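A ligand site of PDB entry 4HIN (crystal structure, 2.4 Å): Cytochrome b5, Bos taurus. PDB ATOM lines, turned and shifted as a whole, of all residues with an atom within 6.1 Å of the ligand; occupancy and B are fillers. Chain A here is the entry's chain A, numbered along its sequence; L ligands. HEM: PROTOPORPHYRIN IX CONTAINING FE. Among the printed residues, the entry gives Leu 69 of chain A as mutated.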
ATOM      1  N   LEU A  21     -31.197   4.274  -5.108  1.00  0.00           N
ATOM      2  CA  LEU A  21     -30.246   4.115  -4.038  1.00  0.00           C
ATOM      3  C   LEU A  21     -30.958   4.085  -2.704  1.00  0.00           C
ATOM      4  O   LEU A  21     -31.946   4.800  -2.516  1.00  0.00           O
ATOM      5  CB  LEU A  21     -29.244   5.278  -4.078  1.00  0.00           C
ATOM      6  CG  LEU A  21     -27.877   4.996  -3.479  1.00  0.00           C
ATOM      7  CD1 LEU A  21     -27.009   4.238  -4.458  1.00  0.00           C
ATOM      8  CD2 LEU A  21     -27.189   6.308  -3.071  1.00  0.00           C
ATOM      9  N   LEU A  23     -30.551   4.815   1.274  1.00  0.00           N
ATOM     10  CA  LEU A  23     -29.817   5.568   2.275  1.00  0.00           C
ATOM     11  C   LEU A  23     -30.668   5.616   3.509  1.00  0.00           C
ATOM     12  O   LEU A  23     -31.755   6.201   3.493  1.00  0.00           O
ATOM     13  CB  LEU A  23     -29.431   6.997   1.810  1.00  0.00           C
ATOM     14  CG  LEU A  23     -28.526   7.126   0.601  1.00  0.00           C
ATOM     15  CD1 LEU A  23     -28.565   8.516   0.046  1.00  0.00           C
ATOM     16  CD2 LEU A  23     -27.095   6.769   0.937  1.00  0.00           C
ATOM     17  N   LEU A  30     -32.345   8.587  -8.294  1.00  0.00           N
ATOM     18  CA  LEU A  30     -31.291   9.546  -8.631  1.00  0.00           C
ATOM     19  C   LEU A  30     -30.891   9.543 -10.120  1.00  0.00           C
ATOM     20  O   LEU A  30     -29.810  10.030 -10.450  1.00  0.00           O
ATOM     21  CB  LEU A  30     -30.062   9.271  -7.753  1.00  0.00           C
ATOM     22  CG  LEU A  30     -30.260   9.366  -6.239  1.00  0.00           C
ATOM     23  CD1 LEU A  30     -29.118   8.708  -5.516  1.00  0.00           C
ATOM     24  CD2 LEU A  30     -30.425  10.811  -5.788  1.00  0.00           C
ATOM     25  N   PHE A  33     -30.114  12.921 -11.316  1.00  0.00           N
ATOM     26  CA  PHE A  33     -29.066  13.526 -10.507  1.00  0.00           C
ATOM     27  C   PHE A  33     -27.641  13.039 -10.847  1.00  0.00           C
ATOM     28  O   PHE A  33     -26.673  13.742 -10.531  1.00  0.00           O
ATOM     29  CB  PHE A  33     -29.341  13.274  -9.012  1.00  0.00           C
ATOM     30  CG  PHE A  33     -28.338  13.887  -8.060  1.00  0.00           C
ATOM     31  CD1 PHE A  33     -28.253  15.261  -7.910  1.00  0.00           C
ATOM     32  CD2 PHE A  33     -27.470  13.090  -7.323  1.00  0.00           C
ATOM     33  CE1 PHE A  33     -27.310  15.829  -7.041  1.00  0.00           C
ATOM     34  CE2 PHE A  33     -26.524  13.658  -6.467  1.00  0.00           C
ATOM     35  CZ  PHE A  33     -26.453  15.023  -6.321  1.00  0.00           C
ATOM     36  N   HIS A  37     -24.220  15.324  -9.776  1.00  0.00           N
ATOM     37  CA  HIS A  37     -23.510  15.000  -8.538  1.00  0.00           C
ATOM     38  C   HIS A  37     -22.076  15.592  -8.490  1.00  0.00           C
ATOM     39  O   HIS A  37     -21.227  15.191  -9.300  1.00  0.00           O
ATOM     40  CB  HIS A  37     -23.460  13.480  -8.334  1.00  0.00           C
ATOM     41  CG  HIS A  37     -22.878  13.078  -7.013  1.00  0.00           C
ATOM     42  ND1 HIS A  37     -21.923  12.076  -6.930  1.00  0.00           N
ATOM     43  CD2 HIS A  37     -23.111  13.562  -5.771  1.00  0.00           C
ATOM     44  CE1 HIS A  37     -21.624  11.977  -5.648  1.00  0.00           C
ATOM     45  NE2 HIS A  37     -22.312  12.855  -4.919  1.00  0.00           N
ATOM     46  N   PRO A  38     -21.786  16.473  -7.500  1.00  0.00           N
ATOM     47  CA  PRO A  38     -20.434  17.056  -7.393  1.00  0.00           C
ATOM     48  C   PRO A  38     -19.308  16.033  -7.155  1.00  0.00           C
ATOM     49  O   PRO A  38     -18.164  16.308  -7.511  1.00  0.00           O
ATOM     50  CB  PRO A  38     -20.549  18.018  -6.207  1.00  0.00           C
ATOM     51  CG  PRO A  38     -22.020  18.334  -6.116  1.00  0.00           C
ATOM     52  CD  PRO A  38     -22.686  17.039  -6.466  1.00  0.00           C
ATOM     53  N   GLY A  39     -19.655  14.870  -6.595  1.00  0.00           N
ATOM     54  CA  GLY A  39     -18.710  13.793  -6.347  1.00  0.00           C
ATOM     55  C   GLY A  39     -18.530  12.818  -7.502  1.00  0.00           C
ATOM     56  O   GLY A  39     -17.849  11.806  -7.351  1.00  0.00           O
ATOM     57  N   GLY A  40     -19.145  13.117  -8.658  1.00  0.00           N
ATOM     58  CA  GLY A  40     -19.048  12.317  -9.882  1.00  0.00           C
ATOM     59  C   GLY A  40     -20.113  11.243 -10.033  1.00  0.00           C
ATOM     60  O   GLY A  40     -20.712  10.807  -9.042  1.00  0.00           O
ATOM     61  N   VAL A  43     -19.148   7.044  -8.486  1.00  0.00           N
ATOM     62  CA  VAL A  43     -19.440   6.645  -7.093  1.00  0.00           C
ATOM     63  C   VAL A  43     -20.920   6.249  -6.930  1.00  0.00           C
ATOM     64  O   VAL A  43     -21.209   5.318  -6.182  1.00  0.00           O
ATOM     65  CB  VAL A  43     -19.031   7.689  -6.025  1.00  0.00           C
ATOM     66  CG1 VAL A  43     -17.507   7.765  -5.883  1.00  0.00           C
ATOM     67  CG2 VAL A  43     -19.634   9.083  -6.295  1.00  0.00           C
ATOM     68  N   LEU A  44     -21.828   6.917  -7.651  1.00  0.00           N
ATOM     69  CA  LEU A  44     -23.254   6.623  -7.618  1.00  0.00           C
ATOM     70  C   LEU A  44     -23.592   5.389  -8.459  1.00  0.00           C
ATOM     71  O   LEU A  44     -24.442   4.600  -8.059  1.00  0.00           O
ATOM     72  CB  LEU A  44     -24.089   7.831  -8.097  1.00  0.00           C
ATOM     73  CG  LEU A  44     -24.042   9.127  -7.279  1.00  0.00           C
ATOM     74  CD1 LEU A  44     -24.981  10.153  -7.870  1.00  0.00           C
ATOM     75  CD2 LEU A  44     -24.441   8.891  -5.838  1.00  0.00           C
ATOM     76  N   GLN A  47     -22.761   1.991  -6.698  1.00  0.00           N
ATOM     77  CA  GLN A  47     -23.694   1.696  -5.609  1.00  0.00           C
ATOM     78  C   GLN A  47     -25.143   1.508  -6.092  1.00  0.00           C
ATOM     79  O   GLN A  47     -25.968   1.047  -5.306  1.00  0.00           O
ATOM     80  CB  GLN A  47     -23.660   2.816  -4.549  1.00  0.00           C
ATOM     81  CG  GLN A  47     -22.302   3.072  -3.870  1.00  0.00           C
ATOM     82  CD  GLN A  47     -21.767   1.888  -3.132  1.00  0.00           C
ATOM     83  OE1 GLN A  47     -22.435   1.299  -2.271  1.00  0.00           O
ATOM     84  NE2 GLN A  47     -20.524   1.546  -3.392  1.00  0.00           N
ATOM     85  N   ALA A  52     -26.154   2.469   0.159  1.00  0.00           N
ATOM     86  CA  ALA A  52     -24.927   3.271   0.143  1.00  0.00           C
ATOM     87  C   ALA A  52     -24.821   4.193   1.371  1.00  0.00           C
ATOM     88  O   ALA A  52     -24.064   5.175   1.338  1.00  0.00           O
ATOM     89  CB  ALA A  52     -24.894   4.088  -1.134  1.00  0.00           C
ATOM     90  N   ASN A  55     -21.170   4.707   2.783  1.00  0.00           N
ATOM     91  CA  ASN A  55     -20.410   5.486   1.797  1.00  0.00           C
ATOM     92  C   ASN A  55     -20.777   6.982   1.824  1.00  0.00           C
ATOM     93  O   ASN A  55     -19.880   7.819   1.758  1.00  0.00           O
ATOM     94  CB  ASN A  55     -20.609   4.924   0.375  1.00  0.00           C
ATOM     95  CG  ASN A  55     -20.156   3.490   0.196  1.00  0.00           C
ATOM     96  OD1 ASN A  55     -20.687   2.784  -0.620  1.00  0.00           O
ATOM     97  ND2 ASN A  55     -19.187   3.018   0.973  1.00  0.00           N
ATOM     98  N   PHE A  56     -22.082   7.291   1.921  1.00  0.00           N
ATOM     99  CA  PHE A  56     -22.592   8.662   1.968  1.00  0.00           C
ATOM    100  C   PHE A  56     -22.124   9.388   3.228  1.00  0.00           C
ATOM    101  O   PHE A  56     -21.677  10.534   3.154  1.00  0.00           O
ATOM    102  CB  PHE A  56     -24.128   8.656   1.882  1.00  0.00           C
ATOM    103  CG  PHE A  56     -24.812   9.996   1.832  1.00  0.00           C
ATOM    104  CD1 PHE A  56     -25.019  10.641   0.606  1.00  0.00           C
ATOM    105  CD2 PHE A  56     -25.288  10.602   2.990  1.00  0.00           C
ATOM    106  CE1 PHE A  56     -25.679  11.890   0.560  1.00  0.00           C
ATOM    107  CE2 PHE A  56     -25.936  11.842   2.925  1.00  0.00           C
ATOM    108  CZ  PHE A  56     -26.139  12.476   1.708  1.00  0.00           C
ATOM    109  N   VAL A  59     -17.873  10.000   3.527  1.00  0.00           N
ATOM    110  CA  VAL A  59     -17.258  11.137   2.830  1.00  0.00           C
ATOM    111  C   VAL A  59     -17.712  12.449   3.467  1.00  0.00           C
ATOM    112  O   VAL A  59     -17.058  13.488   3.335  1.00  0.00           O
ATOM    113  CB  VAL A  59     -17.539  11.133   1.289  1.00  0.00           C
ATOM    114  CG1 VAL A  59     -16.741  10.040   0.577  1.00  0.00           C
ATOM    115  CG2 VAL A  59     -19.023  11.001   0.981  1.00  0.00           C
ATOM    116  N   GLY A  60     -18.856  12.405   4.148  1.00  0.00           N
ATOM    117  CA  GLY A  60     -19.475  13.573   4.747  1.00  0.00           C
ATOM    118  C   GLY A  60     -20.298  14.297   3.713  1.00  0.00           C
ATOM    119  O   GLY A  60     -19.923  14.366   2.533  1.00  0.00           O
ATOM    120  N   HIS A  61     -21.464  14.772   4.121  1.00  0.00           N
ATOM    121  CA  HIS A  61     -22.374  15.525   3.255  1.00  0.00           C
ATOM    122  C   HIS A  61     -23.027  16.640   4.034  1.00  0.00           C
ATOM    123  O   HIS A  61     -23.436  16.433   5.180  1.00  0.00           O
ATOM    124  CB  HIS A  61     -23.429  14.624   2.620  1.00  0.00           C
ATOM    125  CG  HIS A  61     -22.924  13.867   1.437  1.00  0.00           C
ATOM    126  ND1 HIS A  61     -22.347  12.618   1.578  1.00  0.00           N
ATOM    127  CD2 HIS A  61     -22.929  14.205   0.134  1.00  0.00           C
ATOM    128  CE1 HIS A  61     -22.019  12.240   0.356  1.00  0.00           C
ATOM    129  NE2 HIS A  61     -22.328  13.169  -0.540  1.00  0.00           N
ATOM    130  N   SER A  62     -23.120  17.813   3.395  1.00  0.00           N
ATOM    131  CA  SER A  62     -23.696  19.022   3.947  1.00  0.00           C
ATOM    132  C   SER A  62     -25.196  18.886   4.125  1.00  0.00           C
ATOM    133  O   SER A  62     -25.804  17.965   3.563  1.00  0.00           O
ATOM    134  CB  SER A  62     -23.390  20.207   3.041  1.00  0.00           C
ATOM    135  OG  SER A  62     -24.067  20.100   1.796  1.00  0.00           O
ATOM    136  N   THR A  63     -25.821  19.810   4.900  1.00  0.00           N
ATOM    137  CA  THR A  63     -27.268  19.862   5.102  1.00  0.00           C
ATOM    138  C   THR A  63     -27.918  20.177   3.748  1.00  0.00           C
ATOM    139  O   THR A  63     -28.990  19.647   3.467  1.00  0.00           O
ATOM    140  CB  THR A  63     -27.634  20.886   6.195  1.00  0.00           C
ATOM    141  OG1 THR A  63     -27.009  20.506   7.410  1.00  0.00           O
ATOM    142  CG2 THR A  63     -29.138  21.009   6.435  1.00  0.00           C
ATOM    143  N   ASP A  64     -27.237  20.975   2.902  1.00  0.00           N
ATOM    144  CA  ASP A  64     -27.658  21.332   1.542  1.00  0.00           C
ATOM    145  C   ASP A  64     -27.778  20.070   0.677  1.00  0.00           C
ATOM    146  O   ASP A  64     -28.758  19.930  -0.056  1.00  0.00           O
ATOM    147  CB  ASP A  64     -26.677  22.332   0.903  1.00  0.00           C
ATOM    148  CG  ASP A  64     -26.818  23.786   1.375  1.00  0.00           C
ATOM    149  OD1 ASP A  64     -27.759  24.072   2.151  1.00  0.00           O
ATOM    150  OD2 ASP A  64     -25.966  24.625   0.977  1.00  0.00           O
ATOM    151  N   ALA A  65     -26.797  19.147   0.783  1.00  0.00           N
ATOM    152  CA  ALA A  65     -26.767  17.854   0.095  1.00  0.00           C
ATOM    153  C   ALA A  65     -27.916  16.965   0.583  1.00  0.00           C
ATOM    154  O   ALA A  65     -28.514  16.261  -0.228  1.00  0.00           O
ATOM    155  CB  ALA A  65     -25.429  17.154   0.305  1.00  0.00           C
ATOM    156  N   ARG A  66     -28.237  17.030   1.889  1.00  0.00           N
ATOM    157  CA  ARG A  66     -29.297  16.233   2.505  1.00  0.00           C
ATOM    158  C   ARG A  66     -30.693  16.799   2.182  1.00  0.00           C
ATOM    159  O   ARG A  66     -31.642  16.028   2.118  1.00  0.00           O
ATOM    160  CB  ARG A  66     -29.103  16.122   4.022  1.00  0.00           C
ATOM    161  CG  ARG A  66     -27.922  15.242   4.408  1.00  0.00           C
ATOM    162  CD  ARG A  66     -27.469  15.483   5.838  1.00  0.00           C
ATOM    163  NE  ARG A  66     -26.096  15.012   6.041  1.00  0.00           N
ATOM    164  CZ  ARG A  66     -25.771  13.787   6.424  1.00  0.00           C
ATOM    165  NH1 ARG A  66     -26.721  12.886   6.679  1.00  0.00           N
ATOM    166  NH2 ARG A  66     -24.502  13.432   6.543  1.00  0.00           N
ATOM    167  N   LEU A  68     -31.362  18.431  -0.695  1.00  0.00           N
ATOM    168  CA  LEU A  68     -31.449  18.095  -2.112  1.00  0.00           C
ATOM    169  C   LEU A  68     -31.848  16.624  -2.280  1.00  0.00           C
ATOM    170  O   LEU A  68     -32.618  16.280  -3.180  1.00  0.00           O
ATOM    171  CB  LEU A  68     -30.084  18.390  -2.782  1.00  0.00           C
ATOM    172  CG  LEU A  68     -29.928  18.107  -4.281  1.00  0.00           C
ATOM    173  CD1 LEU A  68     -30.832  19.009  -5.143  1.00  0.00           C
ATOM    174  CD2 LEU A  68     -28.492  18.271  -4.687  1.00  0.00           C
ATOM    175  N   LEU A  69     -31.352  15.756  -1.363  1.00  0.00           N
ATOM    176  CA  LEU A  69     -31.613  14.323  -1.296  1.00  0.00           C
ATOM    177  C   LEU A  69     -33.122  14.058  -1.109  1.00  0.00           C
ATOM    178  O   LEU A  69     -33.669  13.198  -1.808  1.00  0.00           O
ATOM    179  CB  LEU A  69     -30.790  13.726  -0.151  1.00  0.00           C
ATOM    180  CG  LEU A  69     -30.763  12.218   0.033  1.00  0.00           C
ATOM    181  CD1 LEU A  69     -30.256  11.503  -1.208  1.00  0.00           C
ATOM    182  CD2 LEU A  69     -29.912  11.850   1.197  1.00  0.00           C
ATOM    183  N   PHE A  72     -35.534  13.661  -4.148  1.00  0.00           N
ATOM    184  CA  PHE A  72     -35.451  12.439  -4.945  1.00  0.00           C
ATOM    185  C   PHE A  72     -36.096  11.214  -4.259  1.00  0.00           C
ATOM    186  O   PHE A  72     -36.138  10.141  -4.860  1.00  0.00           O
ATOM    187  CB  PHE A  72     -33.979  12.140  -5.292  1.00  0.00           C
ATOM    188  CG  PHE A  72     -33.311  13.200  -6.151  1.00  0.00           C
ATOM    189  CD1 PHE A  72     -33.598  13.300  -7.509  1.00  0.00           C
ATOM    190  CD2 PHE A  72     -32.404  14.098  -5.591  1.00  0.00           C
ATOM    191  CE1 PHE A  72     -32.990  14.290  -8.290  1.00  0.00           C
ATOM    192  CE2 PHE A  72     -31.797  15.078  -6.372  1.00  0.00           C
ATOM    193  CZ  PHE A  72     -32.096  15.169  -7.713  1.00  0.00           C
HETATM  194  CHA HEM L   1     -20.124  15.658  -2.749  1.00  0.00           C
HETATM  195  CHB HEM L   1     -19.628  10.926  -2.510  1.00  0.00           C
HETATM  196  CHC HEM L   1     -24.396  10.485  -2.845  1.00  0.00           C
HETATM  197  CHD HEM L   1     -24.865  15.227  -3.098  1.00  0.00           C
HETATM  198  C1A HEM L   1     -19.605  14.395  -2.725  1.00  0.00           C
HETATM  199  C2A HEM L   1     -18.231  14.121  -2.746  1.00  0.00           C
HETATM  200  C3A HEM L   1     -18.081  12.782  -2.695  1.00  0.00           C
HETATM  201  C4A HEM L   1     -19.371  12.251  -2.638  1.00  0.00           C
HETATM  202  CMA HEM L   1     -16.765  12.039  -2.717  1.00  0.00           C
HETATM  203  CAA HEM L   1     -17.085  15.110  -2.868  1.00  0.00           C
HETATM  204  CBA HEM L   1     -16.893  16.101  -1.733  1.00  0.00           C
HETATM  205  CGA HEM L   1     -15.907  15.464  -0.801  1.00  0.00           C
HETATM  206  O1A HEM L   1     -14.757  15.187  -1.143  1.00  0.00           O
HETATM  207  O2A HEM L   1     -16.330  15.194   0.443  1.00  0.00           O
HETATM  208  C1B HEM L   1     -20.914  10.405  -2.467  1.00  0.00           C
HETATM  209  C2B HEM L   1     -21.143   9.009  -2.348  1.00  0.00           C
HETATM  210  C3B HEM L   1     -22.478   8.847  -2.501  1.00  0.00           C
HETATM  211  C4B HEM L   1     -23.041  10.235  -2.643  1.00  0.00           C
HETATM  212  CMB HEM L   1     -20.071   7.960  -2.162  1.00  0.00           C
HETATM  213  CAB HEM L   1     -23.295   7.617  -2.480  1.00  0.00           C
HETATM  214  CBB HEM L   1     -22.957   6.605  -3.266  1.00  0.00           C
HETATM  215  C1C HEM L   1     -24.958  11.722  -2.961  1.00  0.00           C
HETATM  216  C2C HEM L   1     -26.344  11.972  -3.097  1.00  0.00           C
HETATM  217  C3C HEM L   1     -26.500  13.361  -3.142  1.00  0.00           C
HETATM  218  C4C HEM L   1     -25.163  13.896  -3.040  1.00  0.00           C
HETATM  219  CMC HEM L   1     -27.377  10.884  -3.174  1.00  0.00           C
HETATM  220  CAC HEM L   1     -27.727  14.214  -3.247  1.00  0.00           C
HETATM  221  CBC HEM L   1     -28.813  13.907  -3.937  1.00  0.00           C
HETATM  222  C1D HEM L   1     -23.573  15.712  -2.973  1.00  0.00           C
HETATM  223  C2D HEM L   1     -23.331  17.173  -2.934  1.00  0.00           C
HETATM  224  C3D HEM L   1     -22.017  17.316  -2.758  1.00  0.00           C
HETATM  225  C4D HEM L   1     -21.471  15.922  -2.722  1.00  0.00           C
HETATM  226  CMD HEM L   1     -24.383  18.229  -3.027  1.00  0.00           C
HETATM  227  CAD HEM L   1     -21.200  18.600  -2.602  1.00  0.00           C
HETATM  228  CBD HEM L   1     -20.543  18.714  -1.194  1.00  0.00           C
HETATM  229  CGD HEM L   1     -21.576  18.793  -0.072  1.00  0.00           C
HETATM  230  O1D HEM L   1     -21.488  18.109   0.931  1.00  0.00           O
HETATM  231  O2D HEM L   1     -22.623  19.649  -0.190  1.00  0.00           O
HETATM  232  NA  HEM L   1     -20.360  13.243  -2.702  1.00  0.00           N
HETATM  233  NB  HEM L   1     -22.056  11.135  -2.582  1.00  0.00           N
HETATM  234  NC  HEM L   1     -24.233  12.894  -2.919  1.00  0.00           N
HETATM  235  ND  HEM L   1     -22.454  14.992  -2.797  1.00  0.00           N
HETATM  236 FE   HEM L   1     -22.318  13.043  -2.747  1.00  0.00          FE
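N of Ser 62 is in hydrogen-bond range of O1D of the ligand, 3.0 Å away. OG of Ser 62 is in hydrogen-bond range of O2D of the ligand (2.5 Å). FE of the ligand is bound by NE2 of His 61 (2.2 Å). NE2 of His 37 is bound to FE of the ligand, at 2.2 Å.
OG of Ser 62 lies within hydrogen-bond range of N of Ala 65 (3.1 Å). The backbone carbonyl oxygen (O) of His 61 sits at hydrogen-bond distance from the guanidinium group (NE) of Arg 66 (3.1 Å). ND1 of His 37 lies within hydrogen-bond range of O of Gly 40, 2.7 Å away. The backbone NH of Asp 64 lies close to the side-chain hydroxyl of Ser 62 (3.5 Å). ND1 of His 61 is in hydrogen-bond range of O of Phe 56, at 2.7 Å. The side-chain amide oxygen of Asn 55 sits close to the side-chain amide oxygen of Gln 47, 2.8 Å away.
An oxygen (O2A) of the ligand lies close to the backbone carbonyl oxygen (O) of Val 59 (3.4 Å). Merely in contact with the ligand: Phe 33 (3.3 Å), Leu 44 (3.4 Å), Pro 38 (3.5 Å), Phe 56 (3.5 Å), Leu 69 (3.5 Å), Val 43 (3.6 Å), Leu 30 (3.6 Å), Gln 47 (3.6 Å), Gly 39 (3.6 Å), Ala 65 (3.7 Å), Ala 52 (3.8 Å), Asn 55 (3.9 Å) and Phe 72 (3.96 Å). Hydrophobic or aromatic side chains that line the ligand: Leu 30, Phe 33, His 37, Pro 38, Leu 44, Ala 52, Phe 56, Val 59, His 61, Ala 65, Leu 69 and Phe 72.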
